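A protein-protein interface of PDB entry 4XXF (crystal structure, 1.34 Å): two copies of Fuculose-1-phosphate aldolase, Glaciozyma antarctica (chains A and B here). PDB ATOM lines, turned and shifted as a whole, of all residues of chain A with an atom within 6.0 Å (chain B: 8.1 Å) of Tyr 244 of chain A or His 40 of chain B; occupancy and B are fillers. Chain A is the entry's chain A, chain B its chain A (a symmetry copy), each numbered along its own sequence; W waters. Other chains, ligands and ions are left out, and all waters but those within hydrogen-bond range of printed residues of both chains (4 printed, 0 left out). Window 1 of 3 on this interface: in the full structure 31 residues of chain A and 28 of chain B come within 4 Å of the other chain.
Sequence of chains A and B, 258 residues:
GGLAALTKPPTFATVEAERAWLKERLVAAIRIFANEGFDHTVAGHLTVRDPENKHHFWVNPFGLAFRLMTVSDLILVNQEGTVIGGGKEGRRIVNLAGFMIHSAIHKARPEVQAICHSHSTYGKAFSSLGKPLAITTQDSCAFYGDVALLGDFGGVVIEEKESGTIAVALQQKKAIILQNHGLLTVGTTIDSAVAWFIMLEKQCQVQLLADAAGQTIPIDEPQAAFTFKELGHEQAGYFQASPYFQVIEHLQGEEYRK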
ATOM      1  N   ILE A  32       8.259  26.989 -16.726  1.00  0.00           N
ATOM      2  CA  ILE A  32       8.987  26.769 -17.972  1.00  0.00           C
ATOM      3  C   ILE A  32      10.385  26.235 -17.673  1.00  0.00           C
ATOM      4  O   ILE A  32      10.851  25.287 -18.317  1.00  0.00           O
ATOM      5  CB  ILE A  32       9.084  28.070 -18.820  1.00  0.00           C
ATOM      6  CG1 ILE A  32       7.735  28.396 -19.458  1.00  0.00           C
ATOM      7  CG2 ILE A  32      10.199  27.962 -19.869  1.00  0.00           C
ATOM      8  CD1 ILE A  32       7.590  29.850 -19.882  1.00  0.00           C
ATOM      9  N   GLU A  36      11.713  22.731 -19.146  1.00  0.00           N
ATOM     10  CA  GLU A  36      12.921  22.663 -19.974  1.00  0.00           C
ATOM     11  C   GLU A  36      14.045  21.876 -19.303  1.00  0.00           C
ATOM     12  O   GLU A  36      15.070  21.589 -19.934  1.00  0.00           O
ATOM     13  CB  GLU A  36      13.423  24.075 -20.303  1.00  0.00           C
ATOM     14  CG  GLU A  36      12.452  24.910 -21.134  1.00  0.00           C
ATOM     15  CD  GLU A  36      12.247  24.386 -22.539  1.00  0.00           C
ATOM     16  OE1 GLU A  36      13.203  23.847 -23.144  1.00  0.00           O
ATOM     17  OE2 GLU A  36      11.123  24.518 -23.066  1.00  0.00           O
ATOM     18  N   ASP A 139      20.592  32.533 -34.181  1.00  0.00           N
ATOM     19  CA  ASP A 139      20.020  32.686 -32.841  1.00  0.00           C
ATOM     20  C   ASP A 139      21.000  33.324 -31.854  1.00  0.00           C
ATOM     21  O   ASP A 139      20.614  34.161 -31.022  1.00  0.00           O
ATOM     22  CB  ASP A 139      19.564  31.320 -32.309  1.00  0.00           C
ATOM     23  CG  ASP A 139      18.416  30.710 -33.126  1.00  0.00           C
ATOM     24  OD1 ASP A 139      17.516  31.445 -33.585  1.00  0.00           O
ATOM     25  OD2 ASP A 139      18.401  29.477 -33.308  1.00  0.00           O
ATOM     26  N   VAL A 194      13.371  35.521 -19.654  1.00  0.00           N
ATOM     27  CA  VAL A 194      13.182  34.105 -19.926  1.00  0.00           C
ATOM     28  C   VAL A 194      13.651  33.743 -21.334  1.00  0.00           C
ATOM     29  O   VAL A 194      14.356  32.742 -21.502  1.00  0.00           O
ATOM     30  CB  VAL A 194      11.710  33.714 -19.725  1.00  0.00           C
ATOM     31  CG1 VAL A 194      11.425  32.324 -20.277  1.00  0.00           C
ATOM     32  CG2 VAL A 194      11.360  33.737 -18.249  1.00  0.00           C
ATOM     33  N   ILE A 198      16.570  30.942 -22.173  1.00  0.00           N
ATOM     34  CA  ILE A 198      16.333  29.817 -23.077  1.00  0.00           C
ATOM     35  C   ILE A 198      17.316  29.849 -24.248  1.00  0.00           C
ATOM     36  O   ILE A 198      17.903  28.822 -24.627  1.00  0.00           O
ATOM     37  CB  ILE A 198      14.883  29.830 -23.612  1.00  0.00           C
ATOM     38  CG1 ILE A 198      13.905  29.479 -22.490  1.00  0.00           C
ATOM     39  CG2 ILE A 198      14.710  28.845 -24.757  1.00  0.00           C
ATOM     40  CD1 ILE A 198      12.446  29.826 -22.832  1.00  0.00           C
ATOM     41  N   MET A 199      17.494  31.028 -24.837  1.00  0.00           N
ATOM     42  CA  MET A 199      18.364  31.147 -25.999  1.00  0.00           C
ATOM     43  C   MET A 199      19.825  30.957 -25.636  1.00  0.00           C
ATOM     44  O   MET A 199      20.588  30.388 -26.422  1.00  0.00           O
ATOM     45  CB  MET A 199      18.144  32.491 -26.698  1.00  0.00           C
ATOM     46  CG  MET A 199      16.739  32.602 -27.292  1.00  0.00           C
ATOM     47  SD  MET A 199      16.444  34.191 -28.099  1.00  0.00           S
ATOM     48  CE  MET A 199      17.352  33.967 -29.631  1.00  0.00           C
ATOM     49  N   LYS A 202      20.503  27.257 -24.924  1.00  0.00           N
ATOM     50  CA  LYS A 202      20.561  26.557 -26.206  1.00  0.00           C
ATOM     51  C   LYS A 202      21.872  26.820 -26.935  1.00  0.00           C
ATOM     52  O   LYS A 202      22.483  25.880 -27.464  1.00  0.00           O
ATOM     53  CB  LYS A 202      19.377  26.956 -27.091  1.00  0.00           C
ATOM     54  CG  LYS A 202      19.352  26.260 -28.462  1.00  0.00           C
ATOM     55  CD  LYS A 202      19.338  24.738 -28.387  1.00  0.00           C
ATOM     56  CE  LYS A 202      18.076  24.201 -27.720  1.00  0.00           C
ATOM     57  NZ  LYS A 202      18.069  22.709 -27.680  1.00  0.00           N
ATOM     58  N   GLN A 203      22.344  28.067 -26.973  1.00  0.00           N
ATOM     59  CA  GLN A 203      23.578  28.312 -27.696  1.00  0.00           C
ATOM     60  C   GLN A 203      24.778  27.689 -26.973  1.00  0.00           C
ATOM     61  O   GLN A 203      25.726  27.258 -27.629  1.00  0.00           O
ATOM     62  CB  GLN A 203      23.800  29.802 -27.934  1.00  0.00           C
ATOM     63  CG  GLN A 203      25.008  30.069 -28.838  1.00  0.00           C
ATOM     64  CD  GLN A 203      24.915  29.426 -30.214  1.00  0.00           C
ATOM     65  OE1 GLN A 203      23.837  29.272 -30.776  1.00  0.00           O
ATOM     66  NE2 GLN A 203      26.058  29.063 -30.765  1.00  0.00           N
ATOM     67  N   GLN A 240       9.969  36.521 -28.618  1.00  0.00           N
ATOM     68  CA  GLN A 240      10.653  35.237 -28.736  1.00  0.00           C
ATOM     69  C   GLN A 240      10.309  34.279 -27.579  1.00  0.00           C
ATOM     70  O   GLN A 240      10.328  33.060 -27.765  1.00  0.00           O
ATOM     71  CB  GLN A 240      12.168  35.458 -28.842  1.00  0.00           C
ATOM     72  CG  GLN A 240      12.613  35.929 -30.231  1.00  0.00           C
ATOM     73  CD  GLN A 240      14.042  36.456 -30.272  1.00  0.00           C
ATOM     74  OE1 GLN A 240      14.373  37.459 -29.632  1.00  0.00           O
ATOM     75  NE2 GLN A 240      14.893  35.788 -31.034  1.00  0.00           N
ATOM     76  N   ALA A 241       9.954  34.819 -26.414  1.00  0.00           N
ATOM     77  CA  ALA A 241       9.526  33.993 -25.285  1.00  0.00           C
ATOM     78  C   ALA A 241       8.087  33.517 -25.427  1.00  0.00           C
ATOM     79  O   ALA A 241       7.700  32.548 -24.773  1.00  0.00           O
ATOM     80  CB  ALA A 241       9.666  34.762 -23.971  1.00  0.00           C
ATOM     81  N   SER A 242       7.279  34.193 -26.245  1.00  0.00           N
ATOM     82  CA  SER A 242       5.829  33.988 -26.178  1.00  0.00           C
ATOM     83  C   SER A 242       5.343  32.539 -26.402  1.00  0.00           C
ATOM     84  O   SER A 242       4.452  32.110 -25.679  1.00  0.00           O
ATOM     85  CB  SER A 242       5.112  34.965 -27.129  1.00  0.00           C
ATOM     86  OG  SER A 242       5.424  34.765 -28.492  1.00  0.00           O
ATOM     87  N   PRO A 243       5.935  31.768 -27.337  1.00  0.00           N
ATOM     88  CA  PRO A 243       5.409  30.399 -27.473  1.00  0.00           C
ATOM     89  C   PRO A 243       5.638  29.541 -26.220  1.00  0.00           C
ATOM     90  O   PRO A 243       4.820  28.665 -25.932  1.00  0.00           O
ATOM     91  CB  PRO A 243       6.174  29.832 -28.681  1.00  0.00           C
ATOM     92  CG  PRO A 243       7.317  30.754 -28.912  1.00  0.00           C
ATOM     93  CD  PRO A 243       6.925  32.093 -28.381  1.00  0.00           C
ATOM     94  N   TYR A 244       6.695  29.810 -25.459  1.00  0.00           N
ATOM     95  CA  TYR A 244       6.958  29.016 -24.258  1.00  0.00           C
ATOM     96  C   TYR A 244       5.890  29.290 -23.203  1.00  0.00           C
ATOM     97  O   TYR A 244       5.448  28.373 -22.499  1.00  0.00           O
ATOM     98  CB  TYR A 244       8.364  29.302 -23.705  1.00  0.00           C
ATOM     99  CG  TYR A 244       9.458  28.969 -24.693  1.00  0.00           C
ATOM    100  CD1 TYR A 244       9.990  27.684 -24.779  1.00  0.00           C
ATOM    101  CD2 TYR A 244       9.948  29.940 -25.560  1.00  0.00           C
ATOM    102  CE1 TYR A 244      10.985  27.380 -25.716  1.00  0.00           C
ATOM    103  CE2 TYR A 244      10.922  29.652 -26.478  1.00  0.00           C
ATOM    104  CZ  TYR A 244      11.441  28.382 -26.563  1.00  0.00           C
ATOM    105  OH  TYR A 244      12.418  28.117 -27.487  1.00  0.00           O
ATOM    106  N   PHE A 245       5.465  30.547 -23.080  1.00  0.00           N
ATOM    107  CA  PHE A 245       4.383  30.872 -22.161  1.00  0.00           C
ATOM    108  C   PHE A 245       3.043  30.328 -22.632  1.00  0.00           C
ATOM    109  O   PHE A 245       2.246  29.867 -21.816  1.00  0.00           O
ATOM    110  CB  PHE A 245       4.307  32.394 -21.946  1.00  0.00           C
ATOM    111  CG  PHE A 245       5.407  32.924 -21.057  1.00  0.00           C
ATOM    112  CD1 PHE A 245       5.248  32.910 -19.679  1.00  0.00           C
ATOM    113  CD2 PHE A 245       6.612  33.384 -21.587  1.00  0.00           C
ATOM    114  CE1 PHE A 245       6.253  33.383 -18.834  1.00  0.00           C
ATOM    115  CE2 PHE A 245       7.627  33.860 -20.745  1.00  0.00           C
ATOM    116  CZ  PHE A 245       7.444  33.844 -19.361  1.00  0.00           C
ATOM    117  N   GLN A 246       2.789  30.355 -23.936  1.00  0.00           N
ATOM    118  CA  GLN A 246       1.562  29.756 -24.448  1.00  0.00           C
ATOM    119  C   GLN A 246       1.485  28.283 -24.072  1.00  0.00           C
ATOM    120  O   GLN A 246       0.463  27.808 -23.582  1.00  0.00           O
ATOM    121  CB  GLN A 246       1.475  29.879 -25.964  1.00  0.00           C
ATOM    122  CG  GLN A 246       1.378  31.287 -26.518  1.00  0.00           C
ATOM    123  CD  GLN A 246       1.849  31.333 -27.960  1.00  0.00           C
ATOM    124  OE1 GLN A 246       1.755  30.343 -28.687  1.00  0.00           O
ATOM    125  NE2 GLN A 246       2.361  32.480 -28.387  1.00  0.00           N
ATOM    126  N   VAL A 247       2.583  27.567 -24.290  1.00  0.00           N
ATOM    127  CA  VAL A 247       2.591  26.129 -24.060  1.00  0.00           C
ATOM    128  C   VAL A 247       2.486  25.798 -22.576  1.00  0.00           C
ATOM    129  O   VAL A 247       1.711  24.917 -22.198  1.00  0.00           O
ATOM    130  CB  VAL A 247       3.854  25.470 -24.676  1.00  0.00           C
ATOM    131  CG1 VAL A 247       3.979  23.998 -24.233  1.00  0.00           C
ATOM    132  CG2 VAL A 247       3.782  25.543 -26.202  1.00  0.00           C
ATOM    133  N   ILE A 248       3.232  26.491 -21.724  1.00  0.00           N
ATOM    134  CA  ILE A 248       3.198  26.100 -20.321  1.00  0.00           C
ATOM    135  C   ILE A 248       1.815  26.378 -19.702  1.00  0.00           C
ATOM    136  O   ILE A 248       1.365  25.638 -18.815  1.00  0.00           O
ATOM    137  CB  ILE A 248       4.326  26.790 -19.500  1.00  0.00           C
ATOM    138  CG1 ILE A 248       4.628  25.995 -18.219  1.00  0.00           C
ATOM    139  CG2 ILE A 248       3.991  28.236 -19.184  1.00  0.00           C
ATOM    140  CD1 ILE A 248       5.219  24.597 -18.459  1.00  0.00           C
ATOM    141  N   GLU A 249       1.138  27.423 -20.171  1.00  0.00           N
ATOM    142  CA  GLU A 249      -0.214  27.697 -19.698  1.00  0.00           C
ATOM    143  C   GLU A 249      -1.163  26.578 -20.108  1.00  0.00           C
ATOM    144  O   GLU A 249      -1.981  26.118 -19.300  1.00  0.00           O
ATOM    145  CB  GLU A 249      -0.695  29.044 -20.230  1.00  0.00           C
ATOM    146  CG  GLU A 249      -2.063  29.476 -19.703  1.00  0.00           C
ATOM    147  CD  GLU A 249      -2.414  30.891 -20.127  1.00  0.00           C
ATOM    148  OE1 GLU A 249      -3.436  31.063 -20.819  1.00  0.00           O
ATOM    149  OE2 GLU A 249      -1.669  31.834 -19.763  1.00  0.00           O
ATOM    150  N   PHE B  33       7.066  18.701 -35.752  1.00  0.00           N
ATOM    151  CA  PHE B  33       8.256  19.501 -35.431  1.00  0.00           C
ATOM    152  C   PHE B  33       8.300  19.851 -33.945  1.00  0.00           C
ATOM    153  O   PHE B  33       9.351  19.724 -33.318  1.00  0.00           O
ATOM    154  CB  PHE B  33       8.312  20.767 -36.294  1.00  0.00           C
ATOM    155  CG  PHE B  33       8.977  20.564 -37.635  1.00  0.00           C
ATOM    156  CD1 PHE B  33       8.646  19.479 -38.440  1.00  0.00           C
ATOM    157  CD2 PHE B  33       9.935  21.454 -38.093  1.00  0.00           C
ATOM    158  CE1 PHE B  33       9.257  19.285 -39.693  1.00  0.00           C
ATOM    159  CE2 PHE B  33      10.552  21.271 -39.326  1.00  0.00           C
ATOM    160  CZ  PHE B  33      10.205  20.188 -40.141  1.00  0.00           C
ATOM    161  N   ALA B  34       7.169  20.223 -33.362  1.00  0.00           N
ATOM    162  CA  ALA B  34       7.143  20.489 -31.923  1.00  0.00           C
ATOM    163  C   ALA B  34       7.403  19.222 -31.128  1.00  0.00           C
ATOM    164  O   ALA B  34       8.145  19.250 -30.139  1.00  0.00           O
ATOM    165  CB  ALA B  34       5.830  21.097 -31.506  1.00  0.00           C
ATOM    166  N   GLY B  37      10.910  18.363 -30.990  1.00  0.00           N
ATOM    167  CA  GLY B  37      11.732  19.415 -30.411  1.00  0.00           C
ATOM    168  C   GLY B  37      12.553  20.199 -31.418  1.00  0.00           C
ATOM    169  O   GLY B  37      13.580  20.778 -31.051  1.00  0.00           O
ATOM    170  N   PHE B  38      12.099  20.252 -32.669  1.00  0.00           N
ATOM    171  CA  PHE B  38      12.834  20.922 -33.737  1.00  0.00           C
ATOM    172  C   PHE B  38      12.676  22.430 -33.702  1.00  0.00           C
ATOM    173  O   PHE B  38      13.373  23.142 -34.428  1.00  0.00           O
ATOM    174  CB  PHE B  38      12.367  20.449 -35.119  1.00  0.00           C
ATOM    175  CG  PHE B  38      12.700  19.017 -35.447  1.00  0.00           C
ATOM    176  CD1 PHE B  38      13.642  18.284 -34.733  1.00  0.00           C
ATOM    177  CD2 PHE B  38      12.062  18.413 -36.515  1.00  0.00           C
ATOM    178  CE1 PHE B  38      13.918  16.956 -35.086  1.00  0.00           C
ATOM    179  CE2 PHE B  38      12.328  17.103 -36.863  1.00  0.00           C
ATOM    180  CZ  PHE B  38      13.253  16.377 -36.152  1.00  0.00           C
ATOM    181  N   ASP B  39      11.728  22.924 -32.912  1.00  0.00           N
ATOM    182  CA  ASP B  39      11.469  24.358 -32.896  1.00  0.00           C
ATOM    183  C   ASP B  39      12.312  25.063 -31.837  1.00  0.00           C
ATOM    184  O   ASP B  39      12.815  24.457 -30.893  1.00  0.00           O
ATOM    185  CB  ASP B  39       9.967  24.650 -32.708  1.00  0.00           C
ATOM    186  CG  ASP B  39       9.311  23.882 -31.558  1.00  0.00           C
ATOM    187  OD1 ASP B  39       8.158  24.254 -31.239  1.00  0.00           O
ATOM    188  OD2 ASP B  39       9.879  22.922 -30.978  1.00  0.00           O
ATOM    189  N   HIS B  40      12.515  26.354 -32.047  1.00  0.00           N
ATOM    190  CA  HIS B  40      13.223  27.215 -31.106  1.00  0.00           C
ATOM    191  C   HIS B  40      12.624  28.599 -31.265  1.00  0.00           C
ATOM    192  O   HIS B  40      12.405  29.057 -32.397  1.00  0.00           O
ATOM    193  CB  HIS B  40      14.743  27.211 -31.376  1.00  0.00           C
ATOM    194  CG  HIS B  40      15.566  27.892 -30.313  1.00  0.00           C
ATOM    195  ND1 HIS B  40      15.521  27.531 -28.985  1.00  0.00           N
ATOM    196  CD2 HIS B  40      16.472  28.900 -30.395  1.00  0.00           C
ATOM    197  CE1 HIS B  40      16.360  28.285 -28.293  1.00  0.00           C
ATOM    198  NE2 HIS B  40      16.949  29.124 -29.125  1.00  0.00           N
ATOM    199  N   THR B  41      12.322  29.239 -30.138  1.00  0.00           N
ATOM    200  CA  THR B  41      11.665  30.553 -30.086  1.00  0.00           C
ATOM    201  C   THR B  41      10.545  30.648 -31.138  1.00  0.00           C
ATOM    202  O   THR B  41       9.702  29.756 -31.212  1.00  0.00           O
ATOM    203  CB  THR B  41      12.691  31.723 -30.227  1.00  0.00           C
ATOM    204  OG1 THR B  41      13.236  31.753 -31.553  1.00  0.00           O
ATOM    205  CG2 THR B  41      13.819  31.573 -29.196  1.00  0.00           C
ATOM    206  N   VAL B  42      10.532  31.713 -31.943  1.00  0.00           N
ATOM    207  CA  VAL B  42       9.479  31.906 -32.944  1.00  0.00           C
ATOM    208  C   VAL B  42      10.004  31.711 -34.354  1.00  0.00           C
ATOM    209  O   VAL B  42       9.325  32.047 -35.333  1.00  0.00           O
ATOM    210  CB  VAL B  42       8.843  33.305 -32.810  1.00  0.00           C
ATOM    211  CG1 VAL B  42       8.120  33.423 -31.481  1.00  0.00           C
ATOM    212  CG2 VAL B  42       9.904  34.402 -32.960  1.00  0.00           C
ATOM    213  N   ALA B  43      11.210  31.163 -34.456  1.00  0.00           N
ATOM    214  CA  ALA B  43      11.827  30.893 -35.730  1.00  0.00           C
ATOM    215  C   ALA B  43      11.113  29.725 -36.389  1.00  0.00           C
ATOM    216  O   ALA B  43      10.489  28.887 -35.721  1.00  0.00           O
ATOM    217  CB  ALA B  43      13.307  30.583 -35.555  1.00  0.00           C
ATOM    218  N   GLY B  44      11.208  29.655 -37.701  1.00  0.00           N
ATOM    219  CA  GLY B  44      10.677  28.497 -38.375  1.00  0.00           C
ATOM    220  C   GLY B  44       9.383  28.750 -39.098  1.00  0.00           C
ATOM    221  O   GLY B  44       8.469  29.451 -38.644  1.00  0.00           O
ATOM    222  N   GLY B  63       4.667  33.649 -34.353  1.00  0.00           N
ATOM    223  CA  GLY B  63       4.622  33.707 -32.900  1.00  0.00           C
ATOM    224  C   GLY B  63       3.797  32.639 -32.198  1.00  0.00           C
ATOM    225  O   GLY B  63       3.853  32.532 -30.977  1.00  0.00           O
ATOM    226  N   LEU B  64       3.005  31.873 -32.940  1.00  0.00           N
ATOM    227  CA  LEU B  64       2.215  30.813 -32.320  1.00  0.00           C
ATOM    228  C   LEU B  64       3.057  29.545 -32.137  1.00  0.00           C
ATOM    229  O   LEU B  64       3.711  29.072 -33.069  1.00  0.00           O
ATOM    230  CB  LEU B  64       0.973  30.499 -33.161  1.00  0.00           C
ATOM    231  CG  LEU B  64       0.066  29.399 -32.607  1.00  0.00           C
ATOM    232  CD1 LEU B  64      -0.507  29.769 -31.256  1.00  0.00           C
ATOM    233  CD2 LEU B  64      -1.047  29.137 -33.588  1.00  0.00           C
ATOM    234  N   ALA B  65       3.047  28.988 -30.931  1.00  0.00           N
ATOM    235  CA  ALA B  65       3.796  27.778 -30.642  1.00  0.00           C
ATOM    236  C   ALA B  65       3.407  26.657 -31.592  1.00  0.00           C
ATOM    237  O   ALA B  65       2.218  26.373 -31.788  1.00  0.00           O
ATOM    238  CB  ALA B  65       3.551  27.334 -29.220  1.00  0.00           C
ATOM    239  N   PHE B  66       4.407  25.979 -32.152  1.00  0.00           N
ATOM    240  CA  PHE B  66       4.138  24.826 -33.014  1.00  0.00           C
ATOM    241  C   PHE B  66       3.302  23.771 -32.271  1.00  0.00           C
ATOM    242  O   PHE B  66       2.429  23.129 -32.868  1.00  0.00           O
ATOM    243  CB  PHE B  66       5.438  24.187 -33.505  1.00  0.00           C
ATOM    244  CG  PHE B  66       6.157  24.952 -34.593  1.00  0.00           C
ATOM    245  CD1 PHE B  66       5.838  26.264 -34.917  1.00  0.00           C
ATOM    246  CD2 PHE B  66       7.171  24.324 -35.293  1.00  0.00           C
ATOM    247  CE1 PHE B  66       6.532  26.931 -35.925  1.00  0.00           C
ATOM    248  CE2 PHE B  66       7.871  24.979 -36.299  1.00  0.00           C
ATOM    249  CZ  PHE B  66       7.552  26.287 -36.613  1.00  0.00           C
ATOM    250  N   LEU B  68       0.934  24.102 -30.313  1.00  0.00           N
ATOM    251  CA  LEU B  68      -0.477  24.462 -30.206  1.00  0.00           C
ATOM    252  C   LEU B  68      -1.132  24.733 -31.556  1.00  0.00           C
ATOM    253  O   LEU B  68      -2.281  25.171 -31.598  1.00  0.00           O
ATOM    254  CB  LEU B  68      -0.635  25.692 -29.307  1.00  0.00           C
ATOM    255  CG  LEU B  68      -0.004  25.525 -27.920  1.00  0.00           C
ATOM    256  CD1 LEU B  68      -0.046  26.848 -27.156  1.00  0.00           C
ATOM    257  CD2 LEU B  68      -0.688  24.421 -27.101  1.00  0.00           C
ATOM    258  N   SER B 118      13.345  25.187 -39.723  1.00  0.00           N
ATOM    259  CA  SER B 118      13.268  25.392 -38.288  1.00  0.00           C
ATOM    260  C   SER B 118      14.681  25.389 -37.761  1.00  0.00           C
ATOM    261  O   SER B 118      15.565  24.779 -38.367  1.00  0.00           O
ATOM    262  CB  SER B 118      12.436  24.286 -37.631  1.00  0.00           C
ATOM    263  OG  SER B 118      12.100  24.598 -36.292  1.00  0.00           O
ATOM    264  N   HIS B 119      14.910  26.077 -36.647  1.00  0.00           N
ATOM    265  CA  HIS B 119      16.253  26.181 -36.084  1.00  0.00           C
ATOM    266  C   HIS B 119      16.496  25.050 -35.097  1.00  0.00           C
ATOM    267  O   HIS B 119      16.656  25.263 -33.903  1.00  0.00           O
ATOM    268  CB  HIS B 119      16.438  27.546 -35.438  1.00  0.00           C
ATOM    269  CG  HIS B 119      16.401  28.674 -36.422  1.00  0.00           C
ATOM    270  ND1 HIS B 119      16.687  29.976 -36.073  1.00  0.00           N
ATOM    271  CD2 HIS B 119      16.112  28.691 -37.746  1.00  0.00           C
ATOM    272  CE1 HIS B 119      16.567  30.748 -37.140  1.00  0.00           C
ATOM    273  NE2 HIS B 119      16.231  29.993 -38.169  1.00  0.00           N
ATOM    274  N   SER B 120      16.517  23.842 -35.630  1.00  0.00           N
ATOM    275  CA  SER B 120      16.686  22.630 -34.841  1.00  0.00           C
ATOM    276  C   SER B 120      18.115  22.514 -34.345  1.00  0.00           C
ATOM    277  O   SER B 120      19.053  22.974 -34.999  1.00  0.00           O
ATOM    278  CB  SER B 120      16.290  21.404 -35.664  1.00  0.00           C
ATOM    279  OG  SER B 120      16.953  21.404 -36.932  1.00  0.00           O
ATOM    280  N   THR B 121      18.265  21.908 -33.173  1.00  0.00           N
ATOM    281  CA  THR B 121      19.514  21.915 -32.425  1.00  0.00           C
ATOM    282  C   THR B 121      20.704  21.357 -33.186  1.00  0.00           C
ATOM    283  O   THR B 121      21.740  22.010 -33.272  1.00  0.00           O
ATOM    284  CB  THR B 121      19.347  21.112 -31.140  1.00  0.00           C
ATOM    285  OG1 THR B 121      18.299  21.693 -30.350  1.00  0.00           O
ATOM    286  CG2 THR B 121      20.619  21.146 -30.321  1.00  0.00           C
ATOM    287  N   LYS B 124      21.497  23.132 -36.589  1.00  0.00           N
ATOM    288  CA  LYS B 124      22.113  24.402 -36.269  1.00  0.00           C
ATOM    289  C   LYS B 124      23.581  24.219 -35.859  1.00  0.00           C
ATOM    290  O   LYS B 124      24.479  24.883 -36.396  1.00  0.00           O
ATOM    291  CB  LYS B 124      21.296  25.087 -35.168  1.00  0.00           C
ATOM    292  CG  LYS B 124      21.900  26.343 -34.634  1.00  0.00           C
ATOM    293  CD  LYS B 124      20.888  27.186 -33.856  1.00  0.00           C
ATOM    294  CE  LYS B 124      20.141  26.391 -32.813  1.00  0.00           C
ATOM    295  NZ  LYS B 124      19.274  27.313 -32.018  1.00  0.00           N
HETATM  296  O   HOH W   1      13.753  25.838 -27.389  1.00  0.00           O
HETATM  297  O   HOH W   2      14.435  33.859 -32.837  1.00  0.00           O
HETATM  298  O   HOH W   3      21.160  28.480 -30.364  1.00  0.00           O
HETATM  299  O   HOH W   4      19.593  30.265 -29.072  1.00  0.00           O
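The side-chain carboxylate (OD1) of Asp 139 of chain A sits at hydrogen-bond distance from a ring nitrogen (ND1) of His 119 of chain B (3.0 Å). OD2 of Asp 139 of chain A is in salt-bridge range of NZ of Lys 124 of chain B (2.7 Å). The side-chain hydroxyl (OG1) of Thr 121 of chain B is in hydrogen-bond range of the side-chain amino group (NZ) of Lys 202 of chain A (2.9 Å). OH of Tyr 244 of chain A sits at hydrogen-bond distance from ND1 of His 40 of chain B, 3.5 Å away. The backbone NH (N) of Thr 41 of chain B lies within hydrogen-bond range of the side-chain hydroxyl (OH) of Tyr 244 of chain A. The backbone carbonyl oxygen (O) of Gly 63 of chain B lies within hydrogen-bond range of the side-chain amide nitrogen (NE2) of Gln 246 of chain A (3.0 Å). The backbone NH of Ala 65 of chain B sits at hydrogen-bond distance from the side-chain amide oxygen of Gln 246 of chain A (2.9 Å).
The side-chain amide nitrogen (NE2) of Gln 240 of chain A sits close to the side-chain sulfur (SD) of Met 199 of chain A (3.7 Å). The backbone carbonyl oxygen (O) of Ser 242 of chain A sits close to the side-chain amide nitrogen (NE2) of Gln 246 of chain A (3.4 Å).
Among the printed residues, merely in contact across the chains: Pro 243 of chain A with Thr 41 of chain B, Gln 246 of chain A with Leu 64 of chain B, Lys 202 of chain A with His 40 of chain B, Val 247 of chain A with Ala 65 of chain B, Asp 139 of chain A with His 40 of chain B, Pro 243 of chain A with Val 42 of chain B, Gln 246 of chain A with Leu 68 of chain B, Met 199 of chain A with Thr 41 of chain B, Pro 243 of chain A with Ala 65 of chain B, Gln 240 of chain A with Thr 41 of chain B, Ser 242 of chain A with Gly 63 of chain B, Lys 202 of chain A with Lys 124 of chain B, Met 199 of chain A with His 40 of chain B, Ile 198 of chain A with His 40 of chain B and Val 247 of chain A with Leu 68 of chain B.
Of chain B, only His 40 (3.5 Å) and Thr 41 (2.9 Å) come within 4 Å of Tyr 244 of chain A. Of the printed residues of chain A, Ala 65 of chain B touches Pro 243 (3.7 Å), Gln 246 (2.9 Å) and Val 247 (3.5 Å). Of the printed residues of chain A, Leu 64 of chain B touches Gln 246 (3.5 Å). The nearest residue of chain B that does not touch Tyr 244 of chain A is Asp 39 of chain B (5.0 Å). The nearest printed residue of chain A that does not touch Val 42 of chain B is Gln 240 of chain A (4.1 Å).
Hydrophobic or aromatic side chains of chain B that line the printed part of chain A: His 40, Val 42, Leu 64, Ala 65, Leu 68 and His 119. Among the printed residues, Asp or Glu carboxylates within 4 Å of a Lys or Arg side-chain nitrogen of the other chain: Asp 139 of chain A with Lys 124 of chain B.
No position is printed for both chains. Of the 22 pairs that touch across the chains among the printed residues, none has its exchanged pair printed and touching as well.
Water W1 bridges the side-chain hydroxyl (OH) of Tyr 244 of chain A (2.6 Å) and a ring nitrogen (ND1) of His 40 of chain B (2.9 Å). Water W2 bridges NE2 of Gln 240 of chain A and OG1 of Thr 41 of chain B. Water W3 bridges NZ of Lys 124 of chain B (2.8 Å) and OE1 of Gln 203 of chain A (2.8 Å).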
